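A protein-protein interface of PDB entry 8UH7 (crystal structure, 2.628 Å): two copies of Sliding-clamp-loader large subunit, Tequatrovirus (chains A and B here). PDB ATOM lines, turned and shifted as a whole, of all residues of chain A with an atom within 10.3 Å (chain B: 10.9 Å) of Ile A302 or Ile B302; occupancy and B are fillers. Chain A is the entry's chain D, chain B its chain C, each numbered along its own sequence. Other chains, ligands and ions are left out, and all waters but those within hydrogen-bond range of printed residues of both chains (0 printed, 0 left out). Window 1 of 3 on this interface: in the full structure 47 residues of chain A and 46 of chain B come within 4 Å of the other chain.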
ATOM      1  N   PRO A  55      41.507   9.386 -26.910  1.00  0.00           N
ATOM      2  CA  PRO A  55      40.590   9.780 -27.988  1.00  0.00           C
ATOM      3  C   PRO A  55      40.838  11.186 -28.495  1.00  0.00           C
ATOM      4  O   PRO A  55      40.504  11.483 -29.649  1.00  0.00           O
ATOM      5  CB  PRO A  55      39.205   9.648 -27.338  1.00  0.00           C
ATOM      6  CG  PRO A  55      39.465   9.788 -25.872  1.00  0.00           C
ATOM      7  CD  PRO A  55      40.809   9.164 -25.634  1.00  0.00           C
ATOM      8  N   TYR A 266      28.675  22.331 -34.512  1.00  0.00           N
ATOM      9  CA  TYR A 266      27.458  21.868 -33.852  1.00  0.00           C
ATOM     10  C   TYR A 266      27.615  21.834 -32.336  1.00  0.00           C
ATOM     11  O   TYR A 266      26.669  22.144 -31.601  1.00  0.00           O
ATOM     12  CB  TYR A 266      27.073  20.487 -34.382  1.00  0.00           C
ATOM     13  CG  TYR A 266      25.924  19.849 -33.637  1.00  0.00           C
ATOM     14  CD1 TYR A 266      26.148  19.050 -32.520  1.00  0.00           C
ATOM     15  CD2 TYR A 266      24.616  20.042 -34.051  1.00  0.00           C
ATOM     16  CE1 TYR A 266      25.099  18.472 -31.836  1.00  0.00           C
ATOM     17  CE2 TYR A 266      23.561  19.466 -33.372  1.00  0.00           C
ATOM     18  CZ  TYR A 266      23.807  18.682 -32.268  1.00  0.00           C
ATOM     19  OH  TYR A 266      22.753  18.112 -31.596  1.00  0.00           O
ATOM     20  N   SER A 267      28.792  21.432 -31.845  1.00  0.00           N
ATOM     21  CA  SER A 267      29.002  21.339 -30.403  1.00  0.00           C
ATOM     22  C   SER A 267      28.899  22.710 -29.746  1.00  0.00           C
ATOM     23  O   SER A 267      28.150  22.900 -28.772  1.00  0.00           O
ATOM     24  CB  SER A 267      30.364  20.703 -30.120  1.00  0.00           C
ATOM     25  OG  SER A 267      30.687  20.779 -28.744  1.00  0.00           O
ATOM     26  N   VAL A 270      25.128  23.879 -29.850  1.00  0.00           N
ATOM     27  CA  VAL A 270      24.194  23.355 -28.857  1.00  0.00           C
ATOM     28  C   VAL A 270      24.538  23.892 -27.473  1.00  0.00           C
ATOM     29  O   VAL A 270      23.641  24.187 -26.668  1.00  0.00           O
ATOM     30  CB  VAL A 270      24.145  21.815 -28.879  1.00  0.00           C
ATOM     31  CG1 VAL A 270      23.526  21.328 -30.176  1.00  0.00           C
ATOM     32  CG2 VAL A 270      25.523  21.214 -28.676  1.00  0.00           C
ATOM     33  N   VAL A 293      17.240  19.186 -26.183  1.00  0.00           N
ATOM     34  CA  VAL A 293      18.608  19.546 -26.538  1.00  0.00           C
ATOM     35  C   VAL A 293      19.585  18.448 -26.127  1.00  0.00           C
ATOM     36  O   VAL A 293      20.503  18.107 -26.879  1.00  0.00           O
ATOM     37  CB  VAL A 293      18.977  20.905 -25.914  1.00  0.00           C
ATOM     38  CG1 VAL A 293      20.435  21.229 -26.161  1.00  0.00           C
ATOM     39  CG2 VAL A 293      18.100  21.995 -26.488  1.00  0.00           C
ATOM     40  N   GLY A 294      19.402  17.868 -24.938  1.00  0.00           N
ATOM     41  CA  GLY A 294      20.292  16.814 -24.493  1.00  0.00           C
ATOM     42  C   GLY A 294      20.209  15.578 -25.361  1.00  0.00           C
ATOM     43  O   GLY A 294      21.225  14.939 -25.637  1.00  0.00           O
ATOM     44  N   GLU A 295      19.005  15.232 -25.824  1.00  0.00           N
ATOM     45  CA  GLU A 295      18.881  14.101 -26.735  1.00  0.00           C
ATOM     46  C   GLU A 295      19.531  14.409 -28.078  1.00  0.00           C
ATOM     47  O   GLU A 295      20.309  13.600 -28.605  1.00  0.00           O
ATOM     48  CB  GLU A 295      17.412  13.725 -26.911  1.00  0.00           C
ATOM     49  CG  GLU A 295      16.851  12.913 -25.759  1.00  0.00           C
ATOM     50  CD  GLU A 295      15.430  12.466 -26.012  1.00  0.00           C
ATOM     51  OE1 GLU A 295      14.506  13.041 -25.395  1.00  0.00           O
ATOM     52  OE2 GLU A 295      15.235  11.549 -26.837  1.00  0.00           O
ATOM     53  N   ASN A 296      19.235  15.583 -28.643  1.00  0.00           N
ATOM     54  CA  ASN A 296      19.835  15.953 -29.921  1.00  0.00           C
ATOM     55  C   ASN A 296      21.356  15.982 -29.836  1.00  0.00           C
ATOM     56  O   ASN A 296      22.039  15.697 -30.824  1.00  0.00           O
ATOM     57  CB  ASN A 296      19.300  17.310 -30.381  1.00  0.00           C
ATOM     58  CG  ASN A 296      19.514  17.548 -31.863  1.00  0.00           C
ATOM     59  OD1 ASN A 296      20.561  18.039 -32.280  1.00  0.00           O
ATOM     60  ND2 ASN A 296      18.520  17.197 -32.667  1.00  0.00           N
ATOM     61  N   ASN A 297      21.902  16.302 -28.661  1.00  0.00           N
ATOM     62  CA  ASN A 297      23.350  16.359 -28.505  1.00  0.00           C
ATOM     63  C   ASN A 297      23.950  14.979 -28.257  1.00  0.00           C
ATOM     64  O   ASN A 297      25.028  14.670 -28.776  1.00  0.00           O
ATOM     65  CB  ASN A 297      23.709  17.318 -27.370  1.00  0.00           C
ATOM     66  CG  ASN A 297      25.174  17.264 -27.000  1.00  0.00           C
ATOM     67  OD1 ASN A 297      26.035  17.733 -27.744  1.00  0.00           O
ATOM     68  ND2 ASN A 297      25.465  16.699 -25.836  1.00  0.00           N
ATOM     69  N   GLN A 298      23.272  14.133 -27.476  1.00  0.00           N
ATOM     70  CA  GLN A 298      23.784  12.805 -27.158  1.00  0.00           C
ATOM     71  C   GLN A 298      23.570  11.799 -28.278  1.00  0.00           C
ATOM     72  O   GLN A 298      24.099  10.686 -28.196  1.00  0.00           O
ATOM     73  CB  GLN A 298      23.136  12.275 -25.876  1.00  0.00           C
ATOM     74  CG  GLN A 298      21.729  11.737 -26.069  1.00  0.00           C
ATOM     75  CD  GLN A 298      21.086  11.297 -24.764  1.00  0.00           C
ATOM     76  OE1 GLN A 298      21.595  11.580 -23.681  1.00  0.00           O
ATOM     77  NE2 GLN A 298      19.960  10.600 -24.865  1.00  0.00           N
ATOM     78  N   TYR A 299      22.801  12.144 -29.305  1.00  0.00           N
ATOM     79  CA  TYR A 299      22.655  11.282 -30.470  1.00  0.00           C
ATOM     80  C   TYR A 299      23.413  11.808 -31.683  1.00  0.00           C
ATOM     81  O   TYR A 299      23.231  11.287 -32.788  1.00  0.00           O
ATOM     82  CB  TYR A 299      21.175  11.108 -30.811  1.00  0.00           C
ATOM     83  CG  TYR A 299      20.429  10.207 -29.858  1.00  0.00           C
ATOM     84  CD1 TYR A 299      20.903   8.937 -29.560  1.00  0.00           C
ATOM     85  CD2 TYR A 299      19.254  10.629 -29.250  1.00  0.00           C
ATOM     86  CE1 TYR A 299      20.224   8.107 -28.687  1.00  0.00           C
ATOM     87  CE2 TYR A 299      18.568   9.808 -28.374  1.00  0.00           C
ATOM     88  CZ  TYR A 299      19.057   8.549 -28.097  1.00  0.00           C
ATOM     89  OH  TYR A 299      18.378   7.726 -27.227  1.00  0.00           O
ATOM     90  N   HIS A 300      24.267  12.817 -31.504  1.00  0.00           N
ATOM     91  CA  HIS A 300      24.882  13.473 -32.653  1.00  0.00           C
ATOM     92  C   HIS A 300      25.922  12.582 -33.320  1.00  0.00           C
ATOM     93  O   HIS A 300      26.002  12.531 -34.552  1.00  0.00           O
ATOM     94  CB  HIS A 300      25.510  14.798 -32.230  1.00  0.00           C
ATOM     95  CG  HIS A 300      26.279  15.474 -33.319  1.00  0.00           C
ATOM     96  ND1 HIS A 300      27.655  15.457 -33.379  1.00  0.00           N
ATOM     97  CD2 HIS A 300      25.864  16.183 -34.395  1.00  0.00           C
ATOM     98  CE1 HIS A 300      28.056  16.130 -34.442  1.00  0.00           C
ATOM     99  NE2 HIS A 300      26.990  16.579 -35.077  1.00  0.00           N
ATOM    100  N   GLY A 301      26.725  11.873 -32.525  1.00  0.00           N
ATOM    101  CA  GLY A 301      27.773  11.018 -33.060  1.00  0.00           C
ATOM    102  C   GLY A 301      27.280   9.890 -33.947  1.00  0.00           C
ATOM    103  O   GLY A 301      28.103   9.235 -34.599  1.00  0.00           O
ATOM    104  N   ILE A 302      25.972   9.642 -33.987  1.00  0.00           N
ATOM    105  CA  ILE A 302      25.393   8.646 -34.875  1.00  0.00           C
ATOM    106  C   ILE A 302      24.429   9.267 -35.875  1.00  0.00           C
ATOM    107  O   ILE A 302      23.704   8.546 -36.562  1.00  0.00           O
ATOM    108  CB  ILE A 302      24.709   7.518 -34.079  1.00  0.00           C
ATOM    109  CG1 ILE A 302      23.719   8.096 -33.067  1.00  0.00           C
ATOM    110  CG2 ILE A 302      25.749   6.672 -33.379  1.00  0.00           C
ATOM    111  CD1 ILE A 302      23.270   7.104 -32.014  1.00  0.00           C
ATOM    112  N   ALA A 303      24.409  10.594 -35.976  1.00  0.00           N
ATOM    113  CA  ALA A 303      23.564  11.287 -36.939  1.00  0.00           C
ATOM    114  C   ALA A 303      24.336  11.464 -38.242  1.00  0.00           C
ATOM    115  O   ALA A 303      25.394  12.103 -38.260  1.00  0.00           O
ATOM    116  CB  ALA A 303      23.109  12.637 -36.388  1.00  0.00           C
ATOM    117  N   ALA A 304      23.808  10.896 -39.325  1.00  0.00           N
ATOM    118  CA  ALA A 304      24.497  10.965 -40.608  1.00  0.00           C
ATOM    119  C   ALA A 304      24.571  12.398 -41.120  1.00  0.00           C
ATOM    120  O   ALA A 304      25.636  12.864 -41.540  1.00  0.00           O
ATOM    121  CB  ALA A 304      23.796  10.068 -41.627  1.00  0.00           C
ATOM    122  N   ASN A 305      23.449  13.107 -41.090  1.00  0.00           N
ATOM    123  CA  ASN A 305      23.341  14.454 -41.634  1.00  0.00           C
ATOM    124  C   ASN A 305      23.243  15.440 -40.479  1.00  0.00           C
ATOM    125  O   ASN A 305      22.270  15.415 -39.719  1.00  0.00           O
ATOM    126  CB  ASN A 305      22.123  14.565 -42.552  1.00  0.00           C
ATOM    127  CG  ASN A 305      22.123  15.835 -43.377  1.00  0.00           C
ATOM    128  OD1 ASN A 305      22.557  16.895 -42.920  1.00  0.00           O
ATOM    129  ND2 ASN A 305      21.627  15.735 -44.605  1.00  0.00           N
ATOM    130  N   THR A 306      24.248  16.310 -40.356  1.00  0.00           N
ATOM    131  CA  THR A 306      24.265  17.274 -39.261  1.00  0.00           C
ATOM    132  C   THR A 306      23.270  18.406 -39.495  1.00  0.00           C
ATOM    133  O   THR A 306      22.561  18.811 -38.567  1.00  0.00           O
ATOM    134  CB  THR A 306      25.681  17.821 -39.066  1.00  0.00           C
ATOM    135  OG1 THR A 306      26.478  16.849 -38.377  1.00  0.00           O
ATOM    136  CG2 THR A 306      25.664  19.110 -38.264  1.00  0.00           C
ATOM    137  N   HIS A 309      20.020  17.189 -38.709  1.00  0.00           N
ATOM    138  CA  HIS A 309      19.903  17.025 -37.265  1.00  0.00           C
ATOM    139  C   HIS A 309      19.553  18.346 -36.594  1.00  0.00           C
ATOM    140  O   HIS A 309      18.699  18.397 -35.697  1.00  0.00           O
ATOM    141  CB  HIS A 309      21.205  16.461 -36.704  1.00  0.00           C
ATOM    142  CG  HIS A 309      21.035  15.696 -35.431  1.00  0.00           C
ATOM    143  ND1 HIS A 309      20.082  14.713 -35.276  1.00  0.00           N
ATOM    144  CD2 HIS A 309      21.704  15.763 -34.255  1.00  0.00           C
ATOM    145  CE1 HIS A 309      20.167  14.212 -34.056  1.00  0.00           C
ATOM    146  NE2 HIS A 309      21.142  14.832 -33.416  1.00  0.00           N
ATOM    147  N   TYR B 266      35.167  12.175 -17.169  1.00  0.00           N
ATOM    148  CA  TYR B 266      33.747  11.847 -17.130  1.00  0.00           C
ATOM    149  C   TYR B 266      33.493  10.483 -16.503  1.00  0.00           C
ATOM    150  O   TYR B 266      32.544  10.329 -15.730  1.00  0.00           O
ATOM    151  CB  TYR B 266      33.152  11.899 -18.537  1.00  0.00           C
ATOM    152  CG  TYR B 266      31.683  11.547 -18.568  1.00  0.00           C
ATOM    153  CD1 TYR B 266      31.269  10.232 -18.733  1.00  0.00           C
ATOM    154  CD2 TYR B 266      30.709  12.527 -18.424  1.00  0.00           C
ATOM    155  CE1 TYR B 266      29.934   9.900 -18.752  1.00  0.00           C
ATOM    156  CE2 TYR B 266      29.367  12.204 -18.447  1.00  0.00           C
ATOM    157  CZ  TYR B 266      28.988  10.886 -18.609  1.00  0.00           C
ATOM    158  OH  TYR B 266      27.656  10.548 -18.632  1.00  0.00           O
ATOM    159  N   GLY B 294      22.764   5.737 -16.116  1.00  0.00           N
ATOM    160  CA  GLY B 294      23.157   4.734 -17.083  1.00  0.00           C
ATOM    161  C   GLY B 294      22.961   5.199 -18.508  1.00  0.00           C
ATOM    162  O   GLY B 294      23.835   5.001 -19.350  1.00  0.00           O
ATOM    163  N   GLU B 295      21.820   5.834 -18.800  1.00  0.00           N
ATOM    164  CA  GLU B 295      21.616   6.374 -20.141  1.00  0.00           C
ATOM    165  C   GLU B 295      22.671   7.423 -20.466  1.00  0.00           C
ATOM    166  O   GLU B 295      23.279   7.404 -21.549  1.00  0.00           O
ATOM    167  CB  GLU B 295      20.211   6.964 -20.268  1.00  0.00           C
ATOM    168  CG  GLU B 295      19.974   7.703 -21.583  1.00  0.00           C
ATOM    169  CD  GLU B 295      18.598   8.350 -21.668  1.00  0.00           C
ATOM    170  OE1 GLU B 295      17.608   7.710 -21.255  1.00  0.00           O
ATOM    171  OE2 GLU B 295      18.508   9.502 -22.148  1.00  0.00           O
ATOM    172  N   ASN B 296      22.919   8.335 -19.523  1.00  0.00           N
ATOM    173  CA  ASN B 296      23.874   9.411 -19.768  1.00  0.00           C
ATOM    174  C   ASN B 296      25.268   8.857 -20.034  1.00  0.00           C
ATOM    175  O   ASN B 296      25.942   9.271 -20.985  1.00  0.00           O
ATOM    176  CB  ASN B 296      23.886  10.376 -18.584  1.00  0.00           C
ATOM    177  CG  ASN B 296      24.633  11.653 -18.884  1.00  0.00           C
ATOM    178  OD1 ASN B 296      25.809  11.788 -18.557  1.00  0.00           O
ATOM    179  ND2 ASN B 296      23.951  12.601 -19.517  1.00  0.00           N
ATOM    180  N   ASN B 297      25.712   7.903 -19.210  1.00  0.00           N
ATOM    181  CA  ASN B 297      27.027   7.299 -19.401  1.00  0.00           C
ATOM    182  C   ASN B 297      27.081   6.448 -20.664  1.00  0.00           C
ATOM    183  O   ASN B 297      28.132   6.361 -21.307  1.00  0.00           O
ATOM    184  CB  ASN B 297      27.395   6.465 -18.173  1.00  0.00           C
ATOM    185  CG  ASN B 297      28.456   5.427 -18.467  1.00  0.00           C
ATOM    186  OD1 ASN B 297      29.627   5.756 -18.662  1.00  0.00           O
ATOM    187  ND2 ASN B 297      28.052   4.161 -18.490  1.00  0.00           N
ATOM    188  N   GLN B 298      25.962   5.825 -21.037  1.00  0.00           N
ATOM    189  CA  GLN B 298      25.925   5.020 -22.248  1.00  0.00           C
ATOM    190  C   GLN B 298      26.146   5.878 -23.483  1.00  0.00           C
ATOM    191  O   GLN B 298      26.871   5.480 -24.402  1.00  0.00           O
ATOM    192  CB  GLN B 298      24.586   4.284 -22.334  1.00  0.00           C
ATOM    193  CG  GLN B 298      24.244   3.748 -23.709  1.00  0.00           C
ATOM    194  CD  GLN B 298      22.940   2.978 -23.724  1.00  0.00           C
ATOM    195  OE1 GLN B 298      22.696   2.131 -22.864  1.00  0.00           O
ATOM    196  NE2 GLN B 298      22.089   3.273 -24.700  1.00  0.00           N
ATOM    197  N   TYR B 299      25.542   7.062 -23.521  1.00  0.00           N
ATOM    198  CA  TYR B 299      25.656   7.912 -24.696  1.00  0.00           C
ATOM    199  C   TYR B 299      26.855   8.853 -24.637  1.00  0.00           C
ATOM    200  O   TYR B 299      26.901   9.828 -25.393  1.00  0.00           O
ATOM    201  CB  TYR B 299      24.364   8.707 -24.889  1.00  0.00           C
ATOM    202  CG  TYR B 299      23.187   7.845 -25.272  1.00  0.00           C
ATOM    203  CD1 TYR B 299      23.312   6.862 -26.240  1.00  0.00           C
ATOM    204  CD2 TYR B 299      21.954   8.005 -24.659  1.00  0.00           C
ATOM    205  CE1 TYR B 299      22.237   6.069 -26.595  1.00  0.00           C
ATOM    206  CE2 TYR B 299      20.872   7.217 -25.007  1.00  0.00           C
ATOM    207  CZ  TYR B 299      21.019   6.248 -25.977  1.00  0.00           C
ATOM    208  OH  TYR B 299      19.949   5.456 -26.330  1.00  0.00           O
ATOM    209  N   HIS B 300      27.836   8.575 -23.778  1.00  0.00           N
ATOM    210  CA  HIS B 300      28.947   9.508 -23.606  1.00  0.00           C
ATOM    211  C   HIS B 300      29.731   9.687 -24.901  1.00  0.00           C
ATOM    212  O   HIS B 300      29.762  10.778 -25.475  1.00  0.00           O
ATOM    213  CB  HIS B 300      29.875   9.039 -22.487  1.00  0.00           C
ATOM    214  CG  HIS B 300      31.159   9.806 -22.421  1.00  0.00           C
ATOM    215  ND1 HIS B 300      31.239  11.082 -21.905  1.00  0.00           N
ATOM    216  CD2 HIS B 300      32.408   9.492 -22.838  1.00  0.00           C
ATOM    217  CE1 HIS B 300      32.485  11.513 -21.989  1.00  0.00           C
ATOM    218  NE2 HIS B 300      33.214  10.567 -22.552  1.00  0.00           N
ATOM    219  N   GLY B 301      30.366   8.618 -25.381  1.00  0.00           N
ATOM    220  CA  GLY B 301      31.220   8.694 -26.555  1.00  0.00           C
ATOM    221  C   GLY B 301      30.543   9.191 -27.818  1.00  0.00           C
ATOM    222  O   GLY B 301      31.185   9.328 -28.863  1.00  0.00           O
ATOM    223  N   ILE B 302      29.242   9.464 -27.728  1.00  0.00           N
ATOM    224  CA  ILE B 302      28.482   9.997 -28.843  1.00  0.00           C
ATOM    225  C   ILE B 302      28.121  11.468 -28.651  1.00  0.00           C
ATOM    226  O   ILE B 302      28.098  12.221 -29.633  1.00  0.00           O
ATOM    227  CB  ILE B 302      27.214   9.150 -29.074  1.00  0.00           C
ATOM    228  CG1 ILE B 302      27.582   7.736 -29.500  1.00  0.00           C
ATOM    229  CG2 ILE B 302      26.327   9.762 -30.127  1.00  0.00           C
ATOM    230  CD1 ILE B 302      26.372   6.872 -29.757  1.00  0.00           C
ATOM    231  N   ALA B 303      27.858  11.900 -27.418  1.00  0.00           N
ATOM    232  CA  ALA B 303      27.432  13.270 -27.155  1.00  0.00           C
ATOM    233  C   ALA B 303      28.470  14.270 -27.648  1.00  0.00           C
ATOM    234  O   ALA B 303      29.633  14.230 -27.233  1.00  0.00           O
ATOM    235  CB  ALA B 303      27.177  13.455 -25.660  1.00  0.00           C
ATOM    236  N   ALA B 304      28.035  15.175 -28.529  1.00  0.00           N
ATOM    237  CA  ALA B 304      28.955  16.121 -29.152  1.00  0.00           C
ATOM    238  C   ALA B 304      29.502  17.125 -28.144  1.00  0.00           C
ATOM    239  O   ALA B 304      30.660  17.547 -28.249  1.00  0.00           O
ATOM    240  CB  ALA B 304      28.258  16.847 -30.301  1.00  0.00           C
ATOM    241  N   ASN B 305      28.691  17.525 -27.168  1.00  0.00           N
ATOM    242  CA  ASN B 305      29.088  18.515 -26.168  1.00  0.00           C
ATOM    243  C   ASN B 305      28.981  17.864 -24.792  1.00  0.00           C
ATOM    244  O   ASN B 305      27.890  17.789 -24.215  1.00  0.00           O
ATOM    245  CB  ASN B 305      28.226  19.765 -26.274  1.00  0.00           C
ATOM    246  CG  ASN B 305      28.840  20.957 -25.574  1.00  0.00           C
ATOM    247  OD1 ASN B 305      29.369  20.838 -24.470  1.00  0.00           O
ATOM    248  ND2 ASN B 305      28.779  22.119 -26.217  1.00  0.00           N
ATOM    249  N   THR B 306      30.120  17.400 -24.267  1.00  0.00           N
ATOM    250  CA  THR B 306      30.116  16.655 -23.011  1.00  0.00           C
ATOM    251  C   THR B 306      29.665  17.517 -21.841  1.00  0.00           C
ATOM    252  O   THR B 306      29.023  17.015 -20.913  1.00  0.00           O
ATOM    253  CB  THR B 306      31.506  16.080 -22.737  1.00  0.00           C
ATOM    254  OG1 THR B 306      31.963  15.364 -23.892  1.00  0.00           O
ATOM    255  CG2 THR B 306      31.468  15.132 -21.551  1.00  0.00           C
ATOM    256  N   GLU B 307      29.990  18.810 -21.867  1.00  0.00           N
ATOM    257  CA  GLU B 307      29.539  19.709 -20.811  1.00  0.00           C
ATOM    258  C   GLU B 307      28.018  19.827 -20.810  1.00  0.00           C
ATOM    259  O   GLU B 307      27.376  19.754 -19.755  1.00  0.00           O
ATOM    260  CB  GLU B 307      30.196  21.077 -20.988  1.00  0.00           C
ATOM    261  CG  GLU B 307      29.787  22.110 -19.962  1.00  0.00           C
ATOM    262  CD  GLU B 307      30.527  23.420 -20.147  1.00  0.00           C
ATOM    263  OE1 GLU B 307      31.551  23.426 -20.865  1.00  0.00           O
ATOM    264  OE2 GLU B 307      30.089  24.441 -19.575  1.00  0.00           O
ATOM    265  N   LEU B 308      27.425  20.007 -21.993  1.00  0.00           N
ATOM    266  CA  LEU B 308      25.970  20.002 -22.097  1.00  0.00           C
ATOM    267  C   LEU B 308      25.392  18.653 -21.697  1.00  0.00           C
ATOM    268  O   LEU B 308      24.297  18.591 -21.127  1.00  0.00           O
ATOM    269  CB  LEU B 308      25.554  20.367 -23.519  1.00  0.00           C
ATOM    270  CG  LEU B 308      24.093  20.182 -23.919  1.00  0.00           C
ATOM    271  CD1 LEU B 308      23.174  20.947 -22.987  1.00  0.00           C
ATOM    272  CD2 LEU B 308      23.909  20.642 -25.354  1.00  0.00           C
ATOM    273  N   HIS B 309      26.118  17.566 -21.971  1.00  0.00           N
ATOM    274  CA  HIS B 309      25.674  16.241 -21.552  1.00  0.00           C
ATOM    275  C   HIS B 309      25.584  16.153 -20.032  1.00  0.00           C
ATOM    276  O   HIS B 309      24.597  15.653 -19.475  1.00  0.00           O
ATOM    277  CB  HIS B 309      26.634  15.190 -22.107  1.00  0.00           C
ATOM    278  CG  HIS B 309      26.048  13.818 -22.208  1.00  0.00           C
ATOM    279  ND1 HIS B 309      24.865  13.560 -22.865  1.00  0.00           N
ATOM    280  CD2 HIS B 309      26.496  12.622 -21.755  1.00  0.00           C
ATOM    281  CE1 HIS B 309      24.603  12.267 -22.802  1.00  0.00           C
ATOM    282  NE2 HIS B 309      25.577  11.675 -22.135  1.00  0.00           N
ATOM    283  N   LEU B 310      26.611  16.655 -19.339  1.00  0.00           N
ATOM    284  CA  LEU B 310      26.590  16.651 -17.881  1.00  0.00           C
ATOM    285  C   LEU B 310      25.528  17.590 -17.332  1.00  0.00           C
ATOM    286  O   LEU B 310      24.925  17.296 -16.296  1.00  0.00           O
ATOM    287  CB  LEU B 310      27.962  17.027 -17.326  1.00  0.00           C
ATOM    288  CG  LEU B 310      28.920  15.856 -17.112  1.00  0.00           C
ATOM    289  CD1 LEU B 310      30.169  16.327 -16.397  1.00  0.00           C
ATOM    290  CD2 LEU B 310      28.235  14.744 -16.325  1.00  0.00           C
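Of the printed residues of chain A, Ile B302 touches Gln A298 (3.1 Å), Tyr A299 (3.9 Å), His A300 (3.9 Å), Gly A301 (3.2 Å) and Ile A302 (3.7 Å). Of chain A, only Asn A297 (3.2 Å) and Gln A298 (3.7 Å) come within 4 Å of Ala B303. Ala B304 touches just these residues of chain A: Tyr A266 (3.8 Å), Ser A267 (3.3 Å), Asn A297 (3.1 Å) and His A300 (3.4 Å). Of the printed residues of chain B, Tyr A299 touches Tyr B299 (2.9 Å) and Ile B302 (3.9 Å). Of the printed residues of chain A, Tyr B299 touches Gln A298 (3.3 Å) and Tyr A299 (2.9 Å). Of the printed residues of chain B, Tyr A266 touches Ala B304 (3.8 Å). Of the printed residues of chain B, His A300 touches Ile B302 and Ala B304. The nearest residue of chain B that does not touch Ile A302 is Tyr B299 (5.6 Å).
OE2 of Glu B295 is in hydrogen-bond range of NE2 of Gln A298, 3.3 Å away. The side-chain hydroxyl (OH) of Tyr B299 sits at hydrogen-bond distance from the side-chain hydroxyl (OH) of Tyr A299, at 2.9 Å. The backbone NH (N) of Gly A301 lies close to the backbone carbonyl oxygen (O) of Ile B302 (3.2 Å). The side-chain hydroxyl (OG) of Ser A267 is in hydrogen-bond range of the backbone carbonyl oxygen (O) of Ala B304, at 3.3 Å. N of Ala B304 is in hydrogen-bond range of O of Asn A297 (3.1 Å). ND2 of Asn B305 sits at hydrogen-bond distance from O of Ser A267 (2.7 Å). N of Asn B305 sits at hydrogen-bond distance from OD1 of Asn A297 (2.7 Å).
Tyr A266 touches Ala B304, but with the chains exchanged Ala A304 does not touch Tyr B266 (21.1 Å). Gln A298 touches Tyr B299, but with the chains exchanged Tyr A299 does not touch Gln B298 (6.3 Å). Gln A298 touches Ile B302, but with the chains exchanged Ile A302 does not touch Gln B298 (8.3 Å). His A300 touches Ile B302, but with the chains exchanged Ile A302 does not touch His B300 (9.4 Å). Of the 21 pairs that touch across the chains among the printed residues, 2 have their exchanged pair printed and touching as well.
Of the 18 printed residues of chain B, 8 touch a printed residue of chain A. Hydrophobic or aromatic side chains of chain B that line the printed part of chain A: Tyr B299, Ile B302, Ala B303, Ala B304, Leu B308 and His B309. Along chain B the printed residues that touch a printed residue of chain A span positions 295 to 309. Among the printed residues, 21 pairs touch across the chains. Among the printed residues, no Asp or Glu carboxylate lies within 4 Å of a Lys or Arg side-chain nitrogen of the other chain.
Tyr A266 touches Ala B304 (CD1 to CB, 3.8 Å). Leu B308 touches Val A270 (CD2 to CB, 3.7 Å). CG1 of Val A293 touches CD2 of Leu B308, at 3.6 Å. CA of Ala B303 touches O of Asn A297, 3.2 Å away. CD2 of Leu B308 touches CB of Asn A297, 3.9 Å away. Gln A298 touches Ala B303. Gln A298 touches His B309 (OE1 to CE1, 3.2 Å). His A300 touches Ile B302. Ala B304 touches His A300. Ile B302 touches Ile A302.
The backbone carbonyl oxygen (O) of Asn B296 sits at hydrogen-bond distance from a ring nitrogen (NE2) of His B309 (2.7 Å). NE2 of Gln B298 lies close to OH of Tyr B299 (3.5 Å). The backbone NH of Glu B307 lies close to the side-chain amide oxygen of Asn B305 (3.4 Å). N of Leu B308 sits at hydrogen-bond distance from OD1 of Asn B305 (3.3 Å). OH of Tyr A266 lies within hydrogen-bond range of O of Asn A296. NE2 of His A300 is in hydrogen-bond range of OG1 of Thr A306, at 3.4 Å.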
